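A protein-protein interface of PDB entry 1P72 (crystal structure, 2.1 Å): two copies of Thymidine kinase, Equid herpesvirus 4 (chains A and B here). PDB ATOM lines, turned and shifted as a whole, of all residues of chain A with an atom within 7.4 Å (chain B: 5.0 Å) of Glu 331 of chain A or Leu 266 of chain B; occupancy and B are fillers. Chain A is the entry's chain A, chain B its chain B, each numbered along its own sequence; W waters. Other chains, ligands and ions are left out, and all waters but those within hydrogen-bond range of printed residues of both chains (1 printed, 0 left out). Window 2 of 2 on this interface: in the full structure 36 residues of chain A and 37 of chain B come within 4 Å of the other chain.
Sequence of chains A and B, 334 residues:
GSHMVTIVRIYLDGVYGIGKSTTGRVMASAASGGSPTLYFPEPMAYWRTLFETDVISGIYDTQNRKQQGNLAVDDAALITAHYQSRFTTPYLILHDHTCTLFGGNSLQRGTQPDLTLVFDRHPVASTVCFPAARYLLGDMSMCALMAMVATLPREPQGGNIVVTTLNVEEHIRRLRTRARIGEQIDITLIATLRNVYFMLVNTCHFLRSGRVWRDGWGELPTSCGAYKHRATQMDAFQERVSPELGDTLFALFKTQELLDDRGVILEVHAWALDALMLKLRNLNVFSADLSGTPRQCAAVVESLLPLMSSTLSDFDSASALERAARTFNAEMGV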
ATOM      1  N   PRO A  43      13.319  22.473  22.280  1.00  0.00           N
ATOM      2  CA  PRO A  43      13.543  21.518  21.183  1.00  0.00           C
ATOM      3  C   PRO A  43      15.020  21.428  20.708  1.00  0.00           C
ATOM      4  O   PRO A  43      15.329  21.587  19.518  1.00  0.00           O
ATOM      5  CB  PRO A  43      12.628  22.030  20.090  1.00  0.00           C
ATOM      6  CG  PRO A  43      12.595  23.521  20.323  1.00  0.00           C
ATOM      7  CD  PRO A  43      12.655  23.709  21.828  1.00  0.00           C
ATOM      8  N   MET A  44      15.894  21.124  21.664  1.00  0.00           N
ATOM      9  CA  MET A  44      17.347  21.146  21.506  1.00  0.00           C
ATOM     10  C   MET A  44      17.835  20.306  20.330  1.00  0.00           C
ATOM     11  O   MET A  44      18.524  20.831  19.448  1.00  0.00           O
ATOM     12  CB  MET A  44      18.016  20.695  22.818  1.00  0.00           C
ATOM     13  CG  MET A  44      19.344  21.396  23.190  1.00  0.00           C
ATOM     14  SD  MET A  44      19.687  23.053  22.567  1.00  0.00           S
ATOM     15  CE  MET A  44      19.088  24.045  23.913  1.00  0.00           C
ATOM     16  N   ALA A  45      17.469  19.025  20.280  1.00  0.00           N
ATOM     17  CA  ALA A  45      17.905  18.185  19.148  1.00  0.00           C
ATOM     18  C   ALA A  45      17.407  18.690  17.793  1.00  0.00           C
ATOM     19  O   ALA A  45      18.129  18.586  16.796  1.00  0.00           O
ATOM     20  CB  ALA A  45      17.527  16.707  19.347  1.00  0.00           C
ATOM     21  N   TYR A  46      16.181  19.232  17.749  1.00  0.00           N
ATOM     22  CA  TYR A  46      15.663  19.791  16.503  1.00  0.00           C
ATOM     23  C   TYR A  46      16.603  20.900  16.033  1.00  0.00           C
ATOM     24  O   TYR A  46      16.987  20.961  14.852  1.00  0.00           O
ATOM     25  CB  TYR A  46      14.215  20.311  16.645  1.00  0.00           C
ATOM     26  CG  TYR A  46      13.435  20.362  15.331  1.00  0.00           C
ATOM     27  CD1 TYR A  46      12.448  19.416  15.037  1.00  0.00           C
ATOM     28  CD2 TYR A  46      13.697  21.343  14.386  1.00  0.00           C
ATOM     29  CE1 TYR A  46      11.741  19.459  13.838  1.00  0.00           C
ATOM     30  CE2 TYR A  46      12.999  21.404  13.187  1.00  0.00           C
ATOM     31  CZ  TYR A  46      12.039  20.461  12.915  1.00  0.00           C
ATOM     32  OH  TYR A  46      11.369  20.536  11.731  1.00  0.00           O
ATOM     33  N   THR A  49      20.960  18.788  16.394  1.00  0.00           N
ATOM     34  CA  THR A  49      21.432  17.499  15.883  1.00  0.00           C
ATOM     35  C   THR A  49      20.580  16.819  14.808  1.00  0.00           C
ATOM     36  O   THR A  49      21.085  15.966  14.079  1.00  0.00           O
ATOM     37  CB  THR A  49      21.565  16.511  17.034  1.00  0.00           C
ATOM     38  OG1 THR A  49      20.316  16.459  17.728  1.00  0.00           O
ATOM     39  CG2 THR A  49      22.576  16.999  18.086  1.00  0.00           C
ATOM     40  N   LEU A  50      19.291  17.136  14.726  1.00  0.00           N
ATOM     41  CA  LEU A  50      18.432  16.378  13.824  1.00  0.00           C
ATOM     42  C   LEU A  50      18.766  16.624  12.344  1.00  0.00           C
ATOM     43  O   LEU A  50      18.570  15.744  11.525  1.00  0.00           O
ATOM     44  CB  LEU A  50      16.938  16.618  14.109  1.00  0.00           C
ATOM     45  CG  LEU A  50      16.266  16.008  15.356  1.00  0.00           C
ATOM     46  CD1 LEU A  50      14.745  16.084  15.249  1.00  0.00           C
ATOM     47  CD2 LEU A  50      16.736  14.568  15.641  1.00  0.00           C
ATOM     48  N   ALA A 325       4.401  14.455  25.556  1.00  0.00           N
ATOM     49  CA  ALA A 325       5.462  14.869  26.460  1.00  0.00           C
ATOM     50  C   ALA A 325       6.590  13.831  26.460  1.00  0.00           C
ATOM     51  O   ALA A 325       7.765  14.183  26.355  1.00  0.00           O
ATOM     52  CB  ALA A 325       4.914  15.068  27.879  1.00  0.00           C
ATOM     53  N   ARG A 326       6.224  12.561  26.570  1.00  0.00           N
ATOM     54  CA  ARG A 326       7.209  11.472  26.591  1.00  0.00           C
ATOM     55  C   ARG A 326       8.067  11.467  25.315  1.00  0.00           C
ATOM     56  O   ARG A 326       9.292  11.384  25.369  1.00  0.00           O
ATOM     57  CB  ARG A 326       6.500  10.125  26.755  1.00  0.00           C
ATOM     58  CG  ARG A 326       6.755   9.429  28.093  1.00  0.00           C
ATOM     59  CD  ARG A 326       5.584   8.584  28.632  1.00  0.00           C
ATOM     60  NE  ARG A 326       4.775   8.005  27.555  1.00  0.00           N
ATOM     61  CZ  ARG A 326       4.614   6.704  27.337  1.00  0.00           C
ATOM     62  NH1 ARG A 326       5.194   5.800  28.132  1.00  0.00           N
ATOM     63  NH2 ARG A 326       3.866   6.301  26.319  1.00  0.00           N
ATOM     64  N   THR A 327       7.394  11.580  24.174  1.00  0.00           N
ATOM     65  CA  THR A 327       8.013  11.589  22.853  1.00  0.00           C
ATOM     66  C   THR A 327       8.904  12.808  22.605  1.00  0.00           C
ATOM     67  O   THR A 327      10.035  12.695  22.081  1.00  0.00           O
ATOM     68  CB  THR A 327       6.873  11.544  21.817  1.00  0.00           C
ATOM     69  OG1 THR A 327       6.392  10.196  21.738  1.00  0.00           O
ATOM     70  CG2 THR A 327       7.373  11.824  20.473  1.00  0.00           C
ATOM     71  N   PHE A 328       8.389  13.983  22.964  1.00  0.00           N
ATOM     72  CA  PHE A 328       9.124  15.216  22.757  1.00  0.00           C
ATOM     73  C   PHE A 328      10.375  15.236  23.634  1.00  0.00           C
ATOM     74  O   PHE A 328      11.427  15.681  23.192  1.00  0.00           O
ATOM     75  CB  PHE A 328       8.244  16.440  23.065  1.00  0.00           C
ATOM     76  CG  PHE A 328       8.675  17.693  22.361  1.00  0.00           C
ATOM     77  CD1 PHE A 328       9.149  18.780  23.083  1.00  0.00           C
ATOM     78  CD2 PHE A 328       8.596  17.792  20.975  1.00  0.00           C
ATOM     79  CE1 PHE A 328       9.542  19.949  22.441  1.00  0.00           C
ATOM     80  CE2 PHE A 328       8.980  18.966  20.327  1.00  0.00           C
ATOM     81  CZ  PHE A 328       9.455  20.041  21.072  1.00  0.00           C
ATOM     82  N   ASN A 329      10.250  14.765  24.873  1.00  0.00           N
ATOM     83  CA  ASN A 329      11.407  14.672  25.762  1.00  0.00           C
ATOM     84  C   ASN A 329      12.495  13.745  25.200  1.00  0.00           C
ATOM     85  O   ASN A 329      13.666  14.098  25.220  1.00  0.00           O
ATOM     86  CB  ASN A 329      10.996  14.241  27.174  1.00  0.00           C
ATOM     87  CG  ASN A 329      10.618  15.426  28.054  1.00  0.00           C
ATOM     88  OD1 ASN A 329      11.482  16.070  28.654  1.00  0.00           O
ATOM     89  ND2 ASN A 329       9.329  15.743  28.098  1.00  0.00           N
ATOM     90  N   ALA A 330      12.083  12.589  24.680  1.00  0.00           N
ATOM     91  CA  ALA A 330      12.998  11.616  24.084  1.00  0.00           C
ATOM     92  C   ALA A 330      13.665  12.118  22.804  1.00  0.00           C
ATOM     93  O   ALA A 330      14.893  12.066  22.678  1.00  0.00           O
ATOM     94  CB  ALA A 330      12.273  10.275  23.830  1.00  0.00           C
ATOM     95  N   GLU A 331      12.865  12.643  21.872  1.00  0.00           N
ATOM     96  CA  GLU A 331      13.370  13.028  20.545  1.00  0.00           C
ATOM     97  C   GLU A 331      14.142  14.340  20.562  1.00  0.00           C
ATOM     98  O   GLU A 331      14.947  14.588  19.666  1.00  0.00           O
ATOM     99  CB  GLU A 331      12.230  13.091  19.512  1.00  0.00           C
ATOM    100  CG  GLU A 331      11.558  11.749  19.230  1.00  0.00           C
ATOM    101  CD  GLU A 331      10.565  11.781  18.064  1.00  0.00           C
ATOM    102  OE1 GLU A 331      10.103  12.890  17.667  1.00  0.00           O
ATOM    103  OE2 GLU A 331      10.234  10.675  17.552  1.00  0.00           O
ATOM    104  N   MET A 332      13.891  15.185  21.564  1.00  0.00           N
ATOM    105  CA  MET A 332      14.557  16.487  21.641  1.00  0.00           C
ATOM    106  C   MET A 332      15.849  16.521  22.472  1.00  0.00           C
ATOM    107  O   MET A 332      16.608  17.520  22.439  1.00  0.00           O
ATOM    108  CB  MET A 332      13.592  17.582  22.102  1.00  0.00           C
ATOM    109  CG  MET A 332      12.420  17.821  21.125  1.00  0.00           C
ATOM    110  SD  MET A 332      12.928  18.476  19.503  1.00  0.00           S
ATOM    111  CE  MET A 332      12.830  16.976  18.492  1.00  0.00           C
ATOM    112  N   GLY A 333      16.086  15.430  23.199  1.00  0.00           N
ATOM    113  CA  GLY A 333      17.287  15.253  24.002  1.00  0.00           C
ATOM    114  C   GLY A 333      18.555  15.184  23.157  1.00  0.00           C
ATOM    115  O   GLY A 333      18.551  14.700  22.007  1.00  0.00           O
ATOM    116  N   VAL A 334      19.631  15.703  23.747  1.00  0.00           N
ATOM    117  CA  VAL A 334      20.987  15.737  23.168  1.00  0.00           C
ATOM    118  C   VAL A 334      21.111  15.335  21.685  1.00  0.00           C
ATOM    119  O   VAL A 334      20.937  14.168  21.302  1.00  0.00           O
ATOM    120  CB  VAL A 334      22.011  14.972  24.078  1.00  0.00           C
ATOM    121  CG1 VAL A 334      23.422  15.340  23.714  1.00  0.00           C
ATOM    122  CG2 VAL A 334      21.761  15.317  25.529  1.00  0.00           C
ATOM    123  N   LEU B 258      14.560  12.434   7.736  1.00  0.00           N
ATOM    124  CA  LEU B 258      13.423  12.534   8.641  1.00  0.00           C
ATOM    125  C   LEU B 258      13.117  11.232   9.361  1.00  0.00           C
ATOM    126  O   LEU B 258      12.207  11.193  10.193  1.00  0.00           O
ATOM    127  CB  LEU B 258      12.177  13.052   7.899  1.00  0.00           C
ATOM    128  CG  LEU B 258      12.256  14.420   7.206  1.00  0.00           C
ATOM    129  CD1 LEU B 258      10.902  14.775   6.627  1.00  0.00           C
ATOM    130  CD2 LEU B 258      12.780  15.539   8.141  1.00  0.00           C
ATOM    131  N   LEU B 259      13.877  10.179   9.049  1.00  0.00           N
ATOM    132  CA  LEU B 259      13.713   8.877   9.705  1.00  0.00           C
ATOM    133  C   LEU B 259      14.830   8.567  10.731  1.00  0.00           C
ATOM    134  O   LEU B 259      15.934   9.105  10.649  1.00  0.00           O
ATOM    135  CB  LEU B 259      13.623   7.755   8.653  1.00  0.00           C
ATOM    136  CG  LEU B 259      12.882   8.039   7.332  1.00  0.00           C
ATOM    137  CD1 LEU B 259      13.124   6.962   6.280  1.00  0.00           C
ATOM    138  CD2 LEU B 259      11.386   8.251   7.537  1.00  0.00           C
ATOM    139  N   ASP B 260      14.540   7.705  11.702  1.00  0.00           N
ATOM    140  CA  ASP B 260      15.580   7.215  12.608  1.00  0.00           C
ATOM    141  C   ASP B 260      16.408   6.134  11.894  1.00  0.00           C
ATOM    142  O   ASP B 260      16.233   5.926  10.695  1.00  0.00           O
ATOM    143  CB  ASP B 260      15.008   6.727  13.955  1.00  0.00           C
ATOM    144  CG  ASP B 260      13.976   5.612  13.815  1.00  0.00           C
ATOM    145  OD1 ASP B 260      14.029   4.819  12.845  1.00  0.00           O
ATOM    146  OD2 ASP B 260      13.068   5.443  14.663  1.00  0.00           O
ATOM    147  N   VAL B 264      12.172   4.583  10.549  1.00  0.00           N
ATOM    148  CA  VAL B 264      10.878   5.086  11.000  1.00  0.00           C
ATOM    149  C   VAL B 264      10.907   6.599  11.184  1.00  0.00           C
ATOM    150  O   VAL B 264      11.792   7.126  11.862  1.00  0.00           O
ATOM    151  CB  VAL B 264      10.398   4.382  12.296  1.00  0.00           C
ATOM    152  CG1 VAL B 264       8.952   4.762  12.617  1.00  0.00           C
ATOM    153  CG2 VAL B 264      10.503   2.867  12.155  1.00  0.00           C
ATOM    154  N   ILE B 265       9.950   7.289  10.544  1.00  0.00           N
ATOM    155  CA  ILE B 265       9.809   8.738  10.678  1.00  0.00           C
ATOM    156  C   ILE B 265       9.720   9.104  12.146  1.00  0.00           C
ATOM    157  O   ILE B 265       9.012   8.456  12.922  1.00  0.00           O
ATOM    158  CB  ILE B 265       8.583   9.301   9.850  1.00  0.00           C
ATOM    159  CG1 ILE B 265       8.612  10.843   9.781  1.00  0.00           C
ATOM    160  CG2 ILE B 265       7.232   8.755  10.352  1.00  0.00           C
ATOM    161  CD1 ILE B 265       7.617  11.489   8.793  1.00  0.00           C
ATOM    162  N   LEU B 266      10.455  10.142  12.528  1.00  0.00           N
ATOM    163  CA  LEU B 266      10.346  10.678  13.885  1.00  0.00           C
ATOM    164  C   LEU B 266       8.926  11.185  14.137  1.00  0.00           C
ATOM    165  O   LEU B 266       8.235  11.616  13.213  1.00  0.00           O
ATOM    166  CB  LEU B 266      11.352  11.802  14.101  1.00  0.00           C
ATOM    167  CG  LEU B 266      12.846  11.475  14.003  1.00  0.00           C
ATOM    168  CD1 LEU B 266      13.636  12.623  14.644  1.00  0.00           C
ATOM    169  CD2 LEU B 266      13.227  10.114  14.647  1.00  0.00           C
ATOM    170  N   GLU B 267       8.496  11.109  15.390  1.00  0.00           N
ATOM    171  CA  GLU B 267       7.157  11.515  15.764  1.00  0.00           C
ATOM    172  C   GLU B 267       6.952  13.004  15.514  1.00  0.00           C
ATOM    173  O   GLU B 267       5.887  13.411  15.071  1.00  0.00           O
ATOM    174  CB  GLU B 267       6.887  11.173  17.230  1.00  0.00           C
ATOM    175  CG  GLU B 267       6.437   9.732  17.470  1.00  0.00           C
ATOM    176  CD  GLU B 267       5.043   9.448  16.924  1.00  0.00           C
ATOM    177  OE1 GLU B 267       4.052  10.065  17.409  1.00  0.00           O
ATOM    178  OE2 GLU B 267       4.954   8.612  15.992  1.00  0.00           O
ATOM    179  N   VAL B 268       7.979  13.806  15.777  1.00  0.00           N
ATOM    180  CA  VAL B 268       7.895  15.252  15.581  1.00  0.00           C
ATOM    181  C   VAL B 268       7.671  15.599  14.091  1.00  0.00           C
ATOM    182  O   VAL B 268       6.952  16.558  13.775  1.00  0.00           O
ATOM    183  CB  VAL B 268       9.133  15.978  16.208  1.00  0.00           C
ATOM    184  CG1 VAL B 268      10.421  15.605  15.480  1.00  0.00           C
ATOM    185  CG2 VAL B 268       8.946  17.504  16.266  1.00  0.00           C
ATOM    186  N   HIS B 269       8.250  14.804  13.183  1.00  0.00           N
ATOM    187  CA  HIS B 269       8.043  15.022  11.755  1.00  0.00           C
ATOM    188  C   HIS B 269       6.671  14.495  11.307  1.00  0.00           C
ATOM    189  O   HIS B 269       6.021  15.072  10.429  1.00  0.00           O
ATOM    190  CB  HIS B 269       9.165  14.407  10.907  1.00  0.00           C
ATOM    191  CG  HIS B 269      10.552  14.866  11.271  1.00  0.00           C
ATOM    192  ND1 HIS B 269      10.889  16.193  11.431  1.00  0.00           N
ATOM    193  CD2 HIS B 269      11.697  14.163  11.454  1.00  0.00           C
ATOM    194  CE1 HIS B 269      12.177  16.288  11.715  1.00  0.00           C
ATOM    195  NE2 HIS B 269      12.692  15.068  11.733  1.00  0.00           N
ATOM    196  N   ALA B 270       6.245  13.390  11.905  1.00  0.00           N
ATOM    197  CA  ALA B 270       4.898  12.879  11.734  1.00  0.00           C
ATOM    198  C   ALA B 270       3.865  13.947  12.140  1.00  0.00           C
ATOM    199  O   ALA B 270       2.874  14.158  11.438  1.00  0.00           O
ATOM    200  CB  ALA B 270       4.715  11.617  12.548  1.00  0.00           C
HETATM  201  O   HOH W   1       9.597  18.605  11.258  1.00  0.00           O
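Water W1 bridges OH of Tyr 46 of chain A (2.7 Å) and ND1 of His 269 of chain B (2.7 Å).
Tyr 46 of chain A touches His 269 of chain B.
CD1 of Leu 266 of chain B touches CD1 of Leu 50 of chain A, 3.7 Å away.
Thr 327 of chain A touches Glu 267 of chain B.
Leu 266 of chain B touches Glu 331 of chain A (CA to OE2, 3.7 Å).
No position is printed for both chains.
Of the 6 pairs that touch across the chains among the printed residues, none has its exchanged pair printed and touching as well.
The backbone NH (N) of Leu 50 of chain A lies within hydrogen-bond range of the backbone carbonyl oxygen (O) of Ala 45 of chain A.
N of Tyr 46 of chain A sits close to SD of Met 332 of chain A (3.8 Å).
O of Leu 258 of chain B is in hydrogen-bond range of N of Leu 266 of chain B (3.1 Å).
The side-chain carboxylate (OE2) of Glu 331 of chain A lies within hydrogen-bond range of the backbone NH (N) of Glu 267 of chain B, at 2.8 Å.
The side-chain carboxylate (OE1) of Glu 331 of chain A lies within hydrogen-bond range of the backbone NH (N) of Val 268 of chain B (3.0 Å).
Of the 16 printed residues of chain A, 4 touch a printed residue of chain B.
Printed residues of chain A that touch a printed residue of chain B: Tyr 46, Leu 50, Thr 327 and Glu 331.
Hydrophobic or aromatic side chains of chain A within 4 Å of the printed part of chain B: Tyr 46 and Leu 50.
Among the printed residues, 6 pairs touch across the chains.
Among the printed residues, no Asp or Glu carboxylate lies within 4 Å of a Lys or Arg side-chain nitrogen of the other chain.
Of the printed residues of chain B, Tyr 46 of chain A touches His 269.
Glu 331 of chain A touches three residues of chain B.
Leu 266 of chain B touches just these residues of chain A: Leu 50 and Glu 331.
Of the printed residues of chain A, Glu 267 of chain B touches Thr 327 (3.3 Å) and Glu 331 (2.8 Å).
Of the printed residues of chain A, His 269 of chain B touches Tyr 46.
The nearest residue of chain A that does not touch Leu 266 of chain B is Met 332 of chain A (5.9 Å).
The nearest printed residue of chain A that does not touch Glu 267 of chain B is Phe 328 of chain A (6.6 Å).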
